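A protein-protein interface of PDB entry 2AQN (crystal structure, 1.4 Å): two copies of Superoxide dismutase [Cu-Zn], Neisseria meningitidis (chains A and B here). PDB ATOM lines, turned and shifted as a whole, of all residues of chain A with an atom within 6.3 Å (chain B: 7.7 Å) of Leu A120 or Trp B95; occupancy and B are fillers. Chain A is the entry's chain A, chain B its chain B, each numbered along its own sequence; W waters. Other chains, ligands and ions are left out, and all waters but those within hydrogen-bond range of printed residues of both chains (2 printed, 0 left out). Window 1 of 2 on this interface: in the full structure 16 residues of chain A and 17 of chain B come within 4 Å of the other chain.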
ATOM      1  N   SER A  36     -16.259 -27.201   3.373  1.00  0.00           N
ATOM      2  CA  SER A  36     -17.660 -27.167   2.982  1.00  0.00           C
ATOM      3  C   SER A  36     -18.138 -28.596   2.835  1.00  0.00           C
ATOM      4  O   SER A  36     -17.337 -29.514   2.856  1.00  0.00           O
ATOM      5  CB  SER A  36     -17.884 -26.410   1.673  1.00  0.00           C
ATOM      6  OG  SER A  36     -17.586 -27.240   0.565  1.00  0.00           O
ATOM      7  N   ASN A  37     -19.440 -28.759   2.610  1.00  0.00           N
ATOM      8  CA  ASN A  37     -19.970 -30.098   2.395  1.00  0.00           C
ATOM      9  C   ASN A  37     -19.516 -30.687   1.069  1.00  0.00           C
ATOM     10  O   ASN A  37     -19.825 -31.853   0.812  1.00  0.00           O
ATOM     11  CB  ASN A  37     -21.501 -30.040   2.427  1.00  0.00           C
ATOM     12  CG  ASN A  37     -22.049 -29.798   3.810  1.00  0.00           C
ATOM     13  OD1 ASN A  37     -21.332 -29.936   4.782  1.00  0.00           O
ATOM     14  ND2 ASN A  37     -23.297 -29.402   3.955  1.00  0.00           N
ATOM     15  N   TYR A  38     -18.806 -29.922   0.231  1.00  0.00           N
ATOM     16  CA  TYR A  38     -18.406 -30.344  -1.103  1.00  0.00           C
ATOM     17  C   TYR A  38     -16.912 -30.323  -1.282  1.00  0.00           C
ATOM     18  O   TYR A  38     -16.431 -30.602  -2.370  1.00  0.00           O
ATOM     19  CB  TYR A  38     -19.118 -29.483  -2.199  1.00  0.00           C
ATOM     20  CG  TYR A  38     -20.605 -29.805  -2.083  1.00  0.00           C
ATOM     21  CD1 TYR A  38     -21.145 -30.905  -2.721  1.00  0.00           C
ATOM     22  CD2 TYR A  38     -21.449 -29.032  -1.304  1.00  0.00           C
ATOM     23  CE1 TYR A  38     -22.460 -31.214  -2.616  1.00  0.00           C
ATOM     24  CE2 TYR A  38     -22.798 -29.334  -1.174  1.00  0.00           C
ATOM     25  CZ  TYR A  38     -23.293 -30.439  -1.845  1.00  0.00           C
ATOM     26  OH  TYR A  38     -24.625 -30.787  -1.747  1.00  0.00           O
ATOM     27  N   GLY A  39     -16.176 -30.026  -0.230  1.00  0.00           N
ATOM     28  CA  GLY A  39     -14.717 -29.969  -0.334  1.00  0.00           C
ATOM     29  C   GLY A  39     -14.185 -28.675   0.248  1.00  0.00           C
ATOM     30  O   GLY A  39     -14.917 -27.808   0.754  1.00  0.00           O
ATOM     31  N   LEU A  40     -12.867 -28.510   0.164  1.00  0.00           N
ATOM     32  CA  LEU A  40     -12.229 -27.325   0.737  1.00  0.00           C
ATOM     33  C   LEU A  40     -12.430 -26.081  -0.146  1.00  0.00           C
ATOM     34  O   LEU A  40     -12.313 -26.113  -1.371  1.00  0.00           O
ATOM     35  CB  LEU A  40     -10.720 -27.486   0.953  1.00  0.00           C
ATOM     36  CG  LEU A  40     -10.296 -28.626   1.892  1.00  0.00           C
ATOM     37  CD1 LEU A  40      -8.790 -28.576   2.126  1.00  0.00           C
ATOM     38  CD2 LEU A  40     -11.067 -28.565   3.187  1.00  0.00           C
ATOM     39  N   VAL A  41     -12.710 -24.977   0.530  1.00  0.00           N
ATOM     40  CA  VAL A  41     -12.902 -23.685  -0.082  1.00  0.00           C
ATOM     41  C   VAL A  41     -11.728 -22.772   0.253  1.00  0.00           C
ATOM     42  O   VAL A  41     -11.323 -22.635   1.420  1.00  0.00           O
ATOM     43  CB  VAL A  41     -14.223 -23.072   0.386  1.00  0.00           C
ATOM     44  CG1 VAL A  41     -14.370 -21.669  -0.167  1.00  0.00           C
ATOM     45  CG2 VAL A  41     -15.368 -23.970  -0.084  1.00  0.00           C
ATOM     46  N   PHE A  42     -11.186 -22.156  -0.789  1.00  0.00           N
ATOM     47  CA  PHE A  42     -10.035 -21.273  -0.728  1.00  0.00           C
ATOM     48  C   PHE A  42     -10.510 -19.857  -1.000  1.00  0.00           C
ATOM     49  O   PHE A  42     -10.899 -19.528  -2.125  1.00  0.00           O
ATOM     50  CB  PHE A  42      -8.964 -21.664  -1.755  1.00  0.00           C
ATOM     51  CG  PHE A  42      -8.364 -23.036  -1.428  1.00  0.00           C
ATOM     52  CD1 PHE A  42      -9.046 -24.189  -1.748  1.00  0.00           C
ATOM     53  CD2 PHE A  42      -7.126 -23.143  -0.787  1.00  0.00           C
ATOM     54  CE1 PHE A  42      -8.527 -25.399  -1.412  1.00  0.00           C
ATOM     55  CE2 PHE A  42      -6.598 -24.389  -0.461  1.00  0.00           C
ATOM     56  CZ  PHE A  42      -7.314 -25.539  -0.762  1.00  0.00           C
ATOM     57  N   THR A  43     -10.501 -19.011   0.028  1.00  0.00           N
ATOM     58  CA  THR A  43     -11.048 -17.664  -0.080  1.00  0.00           C
ATOM     59  C   THR A  43      -9.899 -16.676  -0.009  1.00  0.00           C
ATOM     60  O   THR A  43      -9.296 -16.473   1.062  1.00  0.00           O
ATOM     61  CB  THR A  43     -12.032 -17.408   1.065  1.00  0.00           C
ATOM     62  OG1 THR A  43     -13.121 -18.336   0.977  1.00  0.00           O
ATOM     63  CG2 THR A  43     -12.630 -15.998   0.937  1.00  0.00           C
ATOM     64  N   PRO A  94      -9.552 -29.430 -11.320  1.00  0.00           N
ATOM     65  CA  PRO A  94      -9.859 -29.672  -9.901  1.00  0.00           C
ATOM     66  C   PRO A  94     -10.836 -30.819  -9.673  1.00  0.00           C
ATOM     67  O   PRO A  94     -10.818 -31.432  -8.580  1.00  0.00           O
ATOM     68  CB  PRO A  94     -10.429 -28.318  -9.474  1.00  0.00           C
ATOM     69  CG  PRO A  94      -9.936 -27.308 -10.460  1.00  0.00           C
ATOM     70  CD  PRO A  94      -9.935 -28.063 -11.753  1.00  0.00           C
ATOM     71  N   TRP A  95     -11.683 -31.130 -10.657  1.00  0.00           N
ATOM     72  CA  TRP A  95     -12.705 -32.149 -10.578  1.00  0.00           C
ATOM     73  C   TRP A  95     -12.294 -33.432 -11.294  1.00  0.00           C
ATOM     74  O   TRP A  95     -13.145 -34.283 -11.578  1.00  0.00           O
ATOM     75  CB  TRP A  95     -14.024 -31.616 -11.173  1.00  0.00           C
ATOM     76  CG  TRP A  95     -13.825 -30.837 -12.444  1.00  0.00           C
ATOM     77  CD1 TRP A  95     -13.748 -31.312 -13.721  1.00  0.00           C
ATOM     78  CD2 TRP A  95     -13.683 -29.411 -12.527  1.00  0.00           C
ATOM     79  NE1 TRP A  95     -13.553 -30.251 -14.593  1.00  0.00           N
ATOM     80  CE2 TRP A  95     -13.513 -29.072 -13.893  1.00  0.00           C
ATOM     81  CE3 TRP A  95     -13.674 -28.382 -11.585  1.00  0.00           C
ATOM     82  CZ2 TRP A  95     -13.341 -27.764 -14.374  1.00  0.00           C
ATOM     83  CZ3 TRP A  95     -13.505 -27.078 -12.053  1.00  0.00           C
ATOM     84  CH2 TRP A  95     -13.339 -26.772 -13.429  1.00  0.00           C
ATOM     85  N   LEU A 104      -5.919 -26.840  -7.966  1.00  0.00           N
ATOM     86  CA  LEU A 104      -7.068 -26.047  -7.543  1.00  0.00           C
ATOM     87  C   LEU A 104      -7.636 -25.294  -8.746  1.00  0.00           C
ATOM     88  O   LEU A 104      -6.930 -25.171  -9.768  1.00  0.00           O
ATOM     89  CB  LEU A 104      -6.676 -25.053  -6.453  1.00  0.00           C
ATOM     90  CG  LEU A 104      -5.857 -25.568  -5.263  1.00  0.00           C
ATOM     91  CD1 LEU A 104      -5.398 -24.417  -4.382  1.00  0.00           C
ATOM     92  CD2 LEU A 104      -6.673 -26.587  -4.478  1.00  0.00           C
ATOM     93  N   PRO A 105      -8.816 -24.713  -8.674  1.00  0.00           N
ATOM     94  CA  PRO A 105      -9.303 -23.817  -9.723  1.00  0.00           C
ATOM     95  C   PRO A 105      -8.372 -22.622  -9.826  1.00  0.00           C
ATOM     96  O   PRO A 105      -7.770 -22.205  -8.832  1.00  0.00           O
ATOM     97  CB  PRO A 105     -10.651 -23.342  -9.182  1.00  0.00           C
ATOM     98  CG  PRO A 105     -11.072 -24.447  -8.227  1.00  0.00           C
ATOM     99  CD  PRO A 105      -9.787 -24.831  -7.561  1.00  0.00           C
ATOM    100  N   PRO A 118     -13.755 -16.715  -3.969  1.00  0.00           N
ATOM    101  CA  PRO A 118     -13.419 -18.028  -3.438  1.00  0.00           C
ATOM    102  C   PRO A 118     -13.568 -19.124  -4.481  1.00  0.00           C
ATOM    103  O   PRO A 118     -14.394 -18.987  -5.377  1.00  0.00           O
ATOM    104  CB  PRO A 118     -14.478 -18.262  -2.363  1.00  0.00           C
ATOM    105  CG  PRO A 118     -15.678 -17.526  -2.875  1.00  0.00           C
ATOM    106  CD  PRO A 118     -15.091 -16.255  -3.482  1.00  0.00           C
ATOM    107  N   VAL A 119     -12.824 -20.218  -4.318  1.00  0.00           N
ATOM    108  CA  VAL A 119     -12.906 -21.334  -5.236  1.00  0.00           C
ATOM    109  C   VAL A 119     -12.917 -22.636  -4.440  1.00  0.00           C
ATOM    110  O   VAL A 119     -12.329 -22.704  -3.341  1.00  0.00           O
ATOM    111  CB  VAL A 119     -11.747 -21.343  -6.254  1.00  0.00           C
ATOM    112  CG1 VAL A 119     -11.726 -20.121  -7.195  1.00  0.00           C
ATOM    113  CG2 VAL A 119     -10.365 -21.456  -5.581  1.00  0.00           C
ATOM    114  N   LEU A 120     -13.563 -23.655  -4.979  1.00  0.00           N
ATOM    115  CA  LEU A 120     -13.741 -24.958  -4.375  1.00  0.00           C
ATOM    116  C   LEU A 120     -12.824 -26.008  -4.970  1.00  0.00           C
ATOM    117  O   LEU A 120     -12.684 -26.138  -6.192  1.00  0.00           O
ATOM    118  CB  LEU A 120     -15.182 -25.401  -4.623  1.00  0.00           C
ATOM    119  CG  LEU A 120     -15.524 -26.829  -4.119  1.00  0.00           C
ATOM    120  CD1 LEU A 120     -15.569 -26.921  -2.596  1.00  0.00           C
ATOM    121  CD2 LEU A 120     -16.831 -27.277  -4.728  1.00  0.00           C
ATOM    122  N   ALA A 121     -12.170 -26.794  -4.121  1.00  0.00           N
ATOM    123  CA  ALA A 121     -11.406 -27.962  -4.549  1.00  0.00           C
ATOM    124  C   ALA A 121     -12.153 -29.203  -4.112  1.00  0.00           C
ATOM    125  O   ALA A 121     -11.973 -29.638  -2.976  1.00  0.00           O
ATOM    126  CB  ALA A 121     -10.027 -27.863  -3.928  1.00  0.00           C
ATOM    127  N   PRO A 122     -12.987 -29.781  -4.951  1.00  0.00           N
ATOM    128  CA  PRO A 122     -13.888 -30.840  -4.458  1.00  0.00           C
ATOM    129  C   PRO A 122     -13.204 -32.146  -4.068  1.00  0.00           C
ATOM    130  O   PRO A 122     -13.801 -32.959  -3.344  1.00  0.00           O
ATOM    131  CB  PRO A 122     -14.781 -31.108  -5.685  1.00  0.00           C
ATOM    132  CG  PRO A 122     -13.885 -30.747  -6.858  1.00  0.00           C
ATOM    133  CD  PRO A 122     -13.179 -29.492  -6.400  1.00  0.00           C
ATOM    134  N   LEU A 124     -10.429 -32.257  -2.314  1.00  0.00           N
ATOM    135  CA  LEU A 124      -9.786 -32.062  -0.990  1.00  0.00           C
ATOM    136  C   LEU A 124     -10.879 -31.987   0.056  1.00  0.00           C
ATOM    137  O   LEU A 124     -11.762 -31.122  -0.003  1.00  0.00           O
ATOM    138  CB  LEU A 124      -8.977 -30.780  -0.982  1.00  0.00           C
ATOM    139  CG  LEU A 124      -7.759 -30.781  -1.922  1.00  0.00           C
ATOM    140  CD1 LEU A 124      -7.082 -29.434  -1.996  1.00  0.00           C
ATOM    141  CD2 LEU A 124      -6.750 -31.816  -1.466  1.00  0.00           C
ATOM    142  N   TYR B  38     -17.785 -34.716  -9.859  1.00  0.00           N
ATOM    143  CA  TYR B  38     -18.016 -33.831  -8.731  1.00  0.00           C
ATOM    144  C   TYR B  38     -19.152 -32.852  -9.010  1.00  0.00           C
ATOM    145  O   TYR B  38     -19.429 -31.983  -8.191  1.00  0.00           O
ATOM    146  CB  TYR B  38     -16.730 -33.056  -8.301  1.00  0.00           C
ATOM    147  CG  TYR B  38     -15.757 -34.131  -7.819  1.00  0.00           C
ATOM    148  CD1 TYR B  38     -15.820 -34.590  -6.505  1.00  0.00           C
ATOM    149  CD2 TYR B  38     -14.839 -34.706  -8.685  1.00  0.00           C
ATOM    150  CE1 TYR B  38     -14.980 -35.567  -6.029  1.00  0.00           C
ATOM    151  CE2 TYR B  38     -13.980 -35.710  -8.231  1.00  0.00           C
ATOM    152  CZ  TYR B  38     -14.074 -36.114  -6.909  1.00  0.00           C
ATOM    153  OH  TYR B  38     -13.227 -37.102  -6.468  1.00  0.00           O
ATOM    154  N   GLY B  92     -26.758 -17.810  -2.029  1.00  0.00           N
ATOM    155  CA  GLY B  92     -25.557 -18.220  -1.332  1.00  0.00           C
ATOM    156  C   GLY B  92     -24.498 -18.804  -2.227  1.00  0.00           C
ATOM    157  O   GLY B  92     -24.337 -18.457  -3.417  1.00  0.00           O
ATOM    158  N   TYR B  93     -23.662 -19.659  -1.631  1.00  0.00           N
ATOM    159  CA  TYR B  93     -22.504 -20.218  -2.320  1.00  0.00           C
ATOM    160  C   TYR B  93     -22.850 -21.426  -3.181  1.00  0.00           C
ATOM    161  O   TYR B  93     -23.840 -22.119  -2.923  1.00  0.00           O
ATOM    162  CB  TYR B  93     -21.378 -20.622  -1.363  1.00  0.00           C
ATOM    163  CG  TYR B  93     -20.755 -19.484  -0.579  1.00  0.00           C
ATOM    164  CD1 TYR B  93     -19.709 -18.754  -1.117  1.00  0.00           C
ATOM    165  CD2 TYR B  93     -21.215 -19.128   0.672  1.00  0.00           C
ATOM    166  CE1 TYR B  93     -19.116 -17.722  -0.451  1.00  0.00           C
ATOM    167  CE2 TYR B  93     -20.646 -18.088   1.366  1.00  0.00           C
ATOM    168  CZ  TYR B  93     -19.603 -17.392   0.803  1.00  0.00           C
ATOM    169  OH  TYR B  93     -19.030 -16.336   1.501  1.00  0.00           O
ATOM    170  N   PRO B  94     -22.026 -21.711  -4.167  1.00  0.00           N
ATOM    171  CA  PRO B  94     -22.281 -22.914  -4.999  1.00  0.00           C
ATOM    172  C   PRO B  94     -22.193 -24.180  -4.165  1.00  0.00           C
ATOM    173  O   PRO B  94     -22.790 -25.187  -4.498  1.00  0.00           O
ATOM    174  CB  PRO B  94     -21.234 -22.835  -6.101  1.00  0.00           C
ATOM    175  CG  PRO B  94     -20.772 -21.408  -6.101  1.00  0.00           C
ATOM    176  CD  PRO B  94     -20.852 -20.964  -4.673  1.00  0.00           C
ATOM    177  N   TRP B  95     -21.445 -24.141  -3.051  1.00  0.00           N
ATOM    178  CA  TRP B  95     -21.241 -25.297  -2.205  1.00  0.00           C
ATOM    179  C   TRP B  95     -22.085 -25.233  -0.929  1.00  0.00           C
ATOM    180  O   TRP B  95     -21.792 -25.969   0.047  1.00  0.00           O
ATOM    181  CB  TRP B  95     -19.758 -25.396  -1.826  1.00  0.00           C
ATOM    182  CG  TRP B  95     -19.132 -24.046  -1.542  1.00  0.00           C
ATOM    183  CD1 TRP B  95     -19.116 -23.377  -0.343  1.00  0.00           C
ATOM    184  CD2 TRP B  95     -18.433 -23.211  -2.486  1.00  0.00           C
ATOM    185  NE1 TRP B  95     -18.459 -22.191  -0.512  1.00  0.00           N
ATOM    186  CE2 TRP B  95     -18.032 -22.067  -1.806  1.00  0.00           C
ATOM    187  CE3 TRP B  95     -18.132 -23.327  -3.841  1.00  0.00           C
ATOM    188  CZ2 TRP B  95     -17.320 -21.031  -2.435  1.00  0.00           C
ATOM    189  CZ3 TRP B  95     -17.423 -22.304  -4.462  1.00  0.00           C
ATOM    190  CH2 TRP B  95     -17.014 -21.150  -3.755  1.00  0.00           C
ATOM    191  N   GLN B  96     -23.099 -24.389  -0.908  1.00  0.00           N
ATOM    192  CA  GLN B  96     -23.980 -24.246   0.253  1.00  0.00           C
ATOM    193  C   GLN B  96     -25.325 -24.906  -0.026  1.00  0.00           C
ATOM    194  O   GLN B  96     -26.030 -24.546  -0.966  1.00  0.00           O
ATOM    195  CB  GLN B  96     -24.187 -22.773   0.550  1.00  0.00           C
ATOM    196  CG  GLN B  96     -25.108 -22.403   1.698  1.00  0.00           C
ATOM    197  CD  GLN B  96     -25.270 -20.886   1.754  1.00  0.00           C
ATOM    198  OE1 GLN B  96     -24.512 -20.104   1.188  1.00  0.00           O
ATOM    199  NE2 GLN B  96     -26.346 -20.460   2.414  1.00  0.00           N
ATOM    200  N   ASP B  97     -25.692 -25.869   0.825  1.00  0.00           N
ATOM    201  CA  ASP B  97     -26.896 -26.651   0.559  1.00  0.00           C
ATOM    202  C   ASP B  97     -28.163 -25.840   0.778  1.00  0.00           C
ATOM    203  O   ASP B  97     -29.134 -26.139   0.064  1.00  0.00           O
ATOM    204  CB  ASP B  97     -26.864 -27.919   1.404  1.00  0.00           C
ATOM    205  CG  ASP B  97     -25.992 -28.992   0.789  1.00  0.00           C
ATOM    206  OD1 ASP B  97     -26.036 -29.165  -0.442  1.00  0.00           O
ATOM    207  OD2 ASP B  97     -25.243 -29.643   1.534  1.00  0.00           O
ATOM    208  N   ASP B  98     -28.155 -24.832   1.656  1.00  0.00           N
ATOM    209  CA  ASP B  98     -29.398 -24.062   1.852  1.00  0.00           C
ATOM    210  C   ASP B  98     -29.405 -22.725   1.111  1.00  0.00           C
ATOM    211  O   ASP B  98     -29.929 -21.684   1.532  1.00  0.00           O
ATOM    212  CB  ASP B  98     -29.706 -23.937   3.353  1.00  0.00           C
ATOM    213  CG  ASP B  98     -28.640 -23.188   4.116  1.00  0.00           C
ATOM    214  OD1 ASP B  98     -27.638 -22.780   3.475  1.00  0.00           O
ATOM    215  OD2 ASP B  98     -28.777 -23.017   5.340  1.00  0.00           O
ATOM    216  N   ALA B  99     -28.834 -22.790  -0.093  1.00  0.00           N
ATOM    217  CA  ALA B  99     -28.843 -21.668  -1.036  1.00  0.00           C
ATOM    218  C   ALA B  99     -29.622 -22.097  -2.272  1.00  0.00           C
ATOM    219  O   ALA B  99     -29.787 -23.305  -2.492  1.00  0.00           O
ATOM    220  CB  ALA B  99     -27.404 -21.259  -1.401  1.00  0.00           C
ATOM    221  N   ASP B 103     -27.407 -21.311  -7.871  1.00  0.00           N
ATOM    222  CA  ASP B 103     -26.244 -20.442  -7.591  1.00  0.00           C
ATOM    223  C   ASP B 103     -24.959 -21.090  -8.049  1.00  0.00           C
ATOM    224  O   ASP B 103     -24.483 -22.056  -7.433  1.00  0.00           O
ATOM    225  CB  ASP B 103     -26.208 -20.123  -6.094  1.00  0.00           C
ATOM    226  CG  ASP B 103     -27.386 -19.256  -5.681  1.00  0.00           C
ATOM    227  OD1 ASP B 103     -28.082 -18.674  -6.561  1.00  0.00           O
ATOM    228  OD2 ASP B 103     -27.634 -19.119  -4.460  1.00  0.00           O
ATOM    229  N   LEU B 104     -24.342 -20.565  -9.112  1.00  0.00           N
ATOM    230  CA  LEU B 104     -23.129 -21.040  -9.718  1.00  0.00           C
ATOM    231  C   LEU B 104     -21.921 -20.197  -9.310  1.00  0.00           C
ATOM    232  O   LEU B 104     -22.092 -19.062  -8.822  1.00  0.00           O
ATOM    233  CB  LEU B 104     -23.211 -21.039 -11.272  1.00  0.00           C
ATOM    234  CG  LEU B 104     -24.446 -21.662 -11.912  1.00  0.00           C
ATOM    235  CD1 LEU B 104     -24.398 -21.541 -13.425  1.00  0.00           C
ATOM    236  CD2 LEU B 104     -24.602 -23.125 -11.519  1.00  0.00           C
ATOM    237  N   PRO B 105     -20.696 -20.681  -9.493  1.00  0.00           N
ATOM    238  CA  PRO B 105     -19.528 -19.830  -9.271  1.00  0.00           C
ATOM    239  C   PRO B 105     -19.560 -18.662 -10.229  1.00  0.00           C
ATOM    240  O   PRO B 105     -20.061 -18.741 -11.345  1.00  0.00           O
ATOM    241  CB  PRO B 105     -18.303 -20.740  -9.572  1.00  0.00           C
ATOM    242  CG  PRO B 105     -18.874 -22.126  -9.315  1.00  0.00           C
ATOM    243  CD  PRO B 105     -20.246 -22.014  -9.915  1.00  0.00           C
ATOM    244  N   ALA B 106     -18.999 -17.567  -9.773  1.00  0.00           N
ATOM    245  CA  ALA B 106     -18.887 -16.369 -10.588  1.00  0.00           C
ATOM    246  C   ALA B 106     -18.022 -16.638 -11.833  1.00  0.00           C
ATOM    247  O   ALA B 106     -17.046 -17.403 -11.837  1.00  0.00           O
ATOM    248  CB  ALA B 106     -18.331 -15.228  -9.750  1.00  0.00           C
ATOM    249  N   LEU B 120     -17.220 -25.228 -11.666  1.00  0.00           N
ATOM    250  CA  LEU B 120     -17.977 -26.372 -11.164  1.00  0.00           C
ATOM    251  C   LEU B 120     -19.129 -25.993 -10.254  1.00  0.00           C
ATOM    252  O   LEU B 120     -18.968 -25.189  -9.345  1.00  0.00           O
ATOM    253  CB  LEU B 120     -17.056 -27.320 -10.385  1.00  0.00           C
ATOM    254  CG  LEU B 120     -17.667 -28.523  -9.711  1.00  0.00           C
ATOM    255  CD1 LEU B 120     -18.038 -29.619 -10.709  1.00  0.00           C
ATOM    256  CD2 LEU B 120     -16.721 -29.111  -8.678  1.00  0.00           C
ATOM    257  N   ALA B 121     -20.288 -26.600 -10.494  1.00  0.00           N
ATOM    258  CA  ALA B 121     -21.472 -26.490  -9.634  1.00  0.00           C
ATOM    259  C   ALA B 121     -21.681 -27.842  -8.934  1.00  0.00           C
ATOM    260  O   ALA B 121     -22.330 -28.779  -9.452  1.00  0.00           O
ATOM    261  CB  ALA B 121     -22.674 -26.056 -10.450  1.00  0.00           C
ATOM    262  N   PRO B 122     -21.082 -28.027  -7.754  1.00  0.00           N
ATOM    263  CA  PRO B 122     -21.072 -29.380  -7.183  1.00  0.00           C
ATOM    264  C   PRO B 122     -22.439 -29.906  -6.761  1.00  0.00           C
ATOM    265  O   PRO B 122     -22.578 -31.112  -6.537  1.00  0.00           O
ATOM    266  CB  PRO B 122     -20.178 -29.218  -5.939  1.00  0.00           C
ATOM    267  CG  PRO B 122     -20.382 -27.777  -5.556  1.00  0.00           C
ATOM    268  CD  PRO B 122     -20.389 -27.059  -6.887  1.00  0.00           C
ATOM    269  N   ARG B 123     -23.444 -29.000  -6.639  1.00  0.00           N
ATOM    270  CA  ARG B 123     -24.729 -29.501  -6.190  1.00  0.00           C
ATOM    271  C   ARG B 123     -25.631 -29.966  -7.336  1.00  0.00           C
ATOM    272  O   ARG B 123     -26.731 -30.463  -7.085  1.00  0.00           O
ATOM    273  CB  ARG B 123     -25.496 -28.427  -5.409  1.00  0.00           C
ATOM    274  CG  ARG B 123     -24.861 -28.111  -4.068  1.00  0.00           C
ATOM    275  CD  ARG B 123     -25.582 -27.129  -3.220  1.00  0.00           C
ATOM    276  NE  ARG B 123     -25.547 -25.753  -3.672  1.00  0.00           N
ATOM    277  CZ  ARG B 123     -26.517 -24.873  -3.744  1.00  0.00           C
ATOM    278  NH1 ARG B 123     -27.794 -25.155  -3.442  1.00  0.00           N
ATOM    279  NH2 ARG B 123     -26.163 -23.661  -4.175  1.00  0.00           N
ATOM    280  N   HIS B 144     -22.127 -14.071  -3.017  1.00  0.00           N
ATOM    281  CA  HIS B 144     -22.746 -15.296  -2.528  1.00  0.00           C
ATOM    282  C   HIS B 144     -23.492 -15.073  -1.219  1.00  0.00           C
ATOM    283  O   HIS B 144     -23.523 -15.944  -0.312  1.00  0.00           O
ATOM    284  CB  HIS B 144     -21.688 -16.423  -2.410  1.00  0.00           C
ATOM    285  CG  HIS B 144     -21.147 -16.810  -3.768  1.00  0.00           C
ATOM    286  ND1 HIS B 144     -19.912 -16.674  -4.267  1.00  0.00           N
ATOM    287  CD2 HIS B 144     -21.876 -17.357  -4.815  1.00  0.00           C
ATOM    288  CE1 HIS B 144     -19.869 -17.118  -5.525  1.00  0.00           C
ATOM    289  NE2 HIS B 144     -21.072 -17.554  -5.894  1.00  0.00           N
HETATM  290  O   HOH W   1     -21.338 -26.617   2.600  1.00  0.00           O
HETATM  291  O   HOH W   2     -24.374 -32.155   1.261  1.00  0.00           O
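ND2 of Asn A37 sits at hydrogen-bond distance from OD2 of Asp B97 (3.1 Å). The side-chain hydroxyl of Tyr A38 sits at hydrogen-bond distance from the side-chain carboxylate of Asp B97 (2.5 Å).
N of Tyr A38 sits at hydrogen-bond distance from OG of Ser A36 (3.0 Å). The side-chain hydroxyl (OG) of Ser A36 lies within hydrogen-bond range of the backbone carbonyl oxygen (O) of Gly A39, 2.7 Å away. The guanidinium group (NH2) of Arg B123 sits at hydrogen-bond distance from the backbone carbonyl oxygen (O) of Tyr B93 (3.1 Å). The backbone carbonyl oxygen (O) of Pro B94 lies within hydrogen-bond range of the guanidinium group (NE) of Arg B123, at 2.9 Å. The backbone carbonyl oxygen (O) of Gln B96 lies close to the guanidinium group (NE) of Arg B123 (3.0 Å). The backbone carbonyl oxygen (O) of Ala B99 lies within hydrogen-bond range of the guanidinium group (NH1) of Arg B123, at 2.9 Å.
Trp B95 touches Ser A36. Trp B95 touches Tyr A38 (O to CD2, 3.4 Å). CG of Arg B123 touches OH of Tyr A38 (3.6 Å). Val A41 touches Trp B95 (CG2 to NE1, 3.6 Å). CD2 of Tyr B38 touches O of Trp A95 (3.4 Å). Trp A95 touches Leu B120. Pro A118 touches Trp B95 (O to CH2, 3.8 Å). CD2 of Leu A120 touches CG of Pro B122, 3.7 Å away. Tyr B38 touches Pro A122. CG of Pro A122 touches CD2 of Leu B120, at 3.7 Å.
Of the printed residues of chain B, Pro A118 touches Trp B95. Printed residues of chain B within 4 Å of Pro A122: Tyr B38 (3.7 Å) and Leu B120 (3.7 Å). Printed residues of chain A within 4 Å of Tyr B38: Trp A95 (3.4 Å) and Pro A122 (3.7 Å). Pro B94 touches none of the printed residues of chain A. Printed residues of chain A within 4 Å of Pro B122: Tyr A38 and Leu A120. The nearest printed residue of chain B that does not touch Ser A36 is Gln B96 (6.2 Å).
Of the 18 printed residues of chain B, 6 touch a printed residue of chain A. Hydrophobic or aromatic side chains of chain B that line the printed part of chain A: Tyr B38, Trp B95, Leu B120 and Pro B122. Printed residues of chain A that touch a printed residue of chain B: Ser A36, Asn A37, Tyr A38, Val A41, Trp A95, Pro A118, Leu A120 and Pro A122. Among the printed residues, no Asp or Glu carboxylate lies within 4 Å of a Lys or Arg side-chain nitrogen of the other chain.
Tyr A38 touches Trp B95, and with the chains exchanged Trp A95 touches Tyr B38. Tyr A38 touches Pro B122, and with the chains exchanged Pro A122 touches Tyr B38. Trp A95 touches Leu B120, and with the chains exchanged Leu A120 touches Trp B95. Leu A120 touches Pro B122, and with the chains exchanged Pro A122 touches Leu B120. Positions printed for both chains: 38, 94, 95, 104, 105, 120, 121 and 122.
Water W2 lies within hydrogen-bond range of OD2 of Asp B97 (2.7 Å) and OH of Tyr A38 (3.3 Å). Water W1 lies within hydrogen-bond range of O of Trp B95 (2.7 Å) and N of Asn A37 (2.9 Å).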
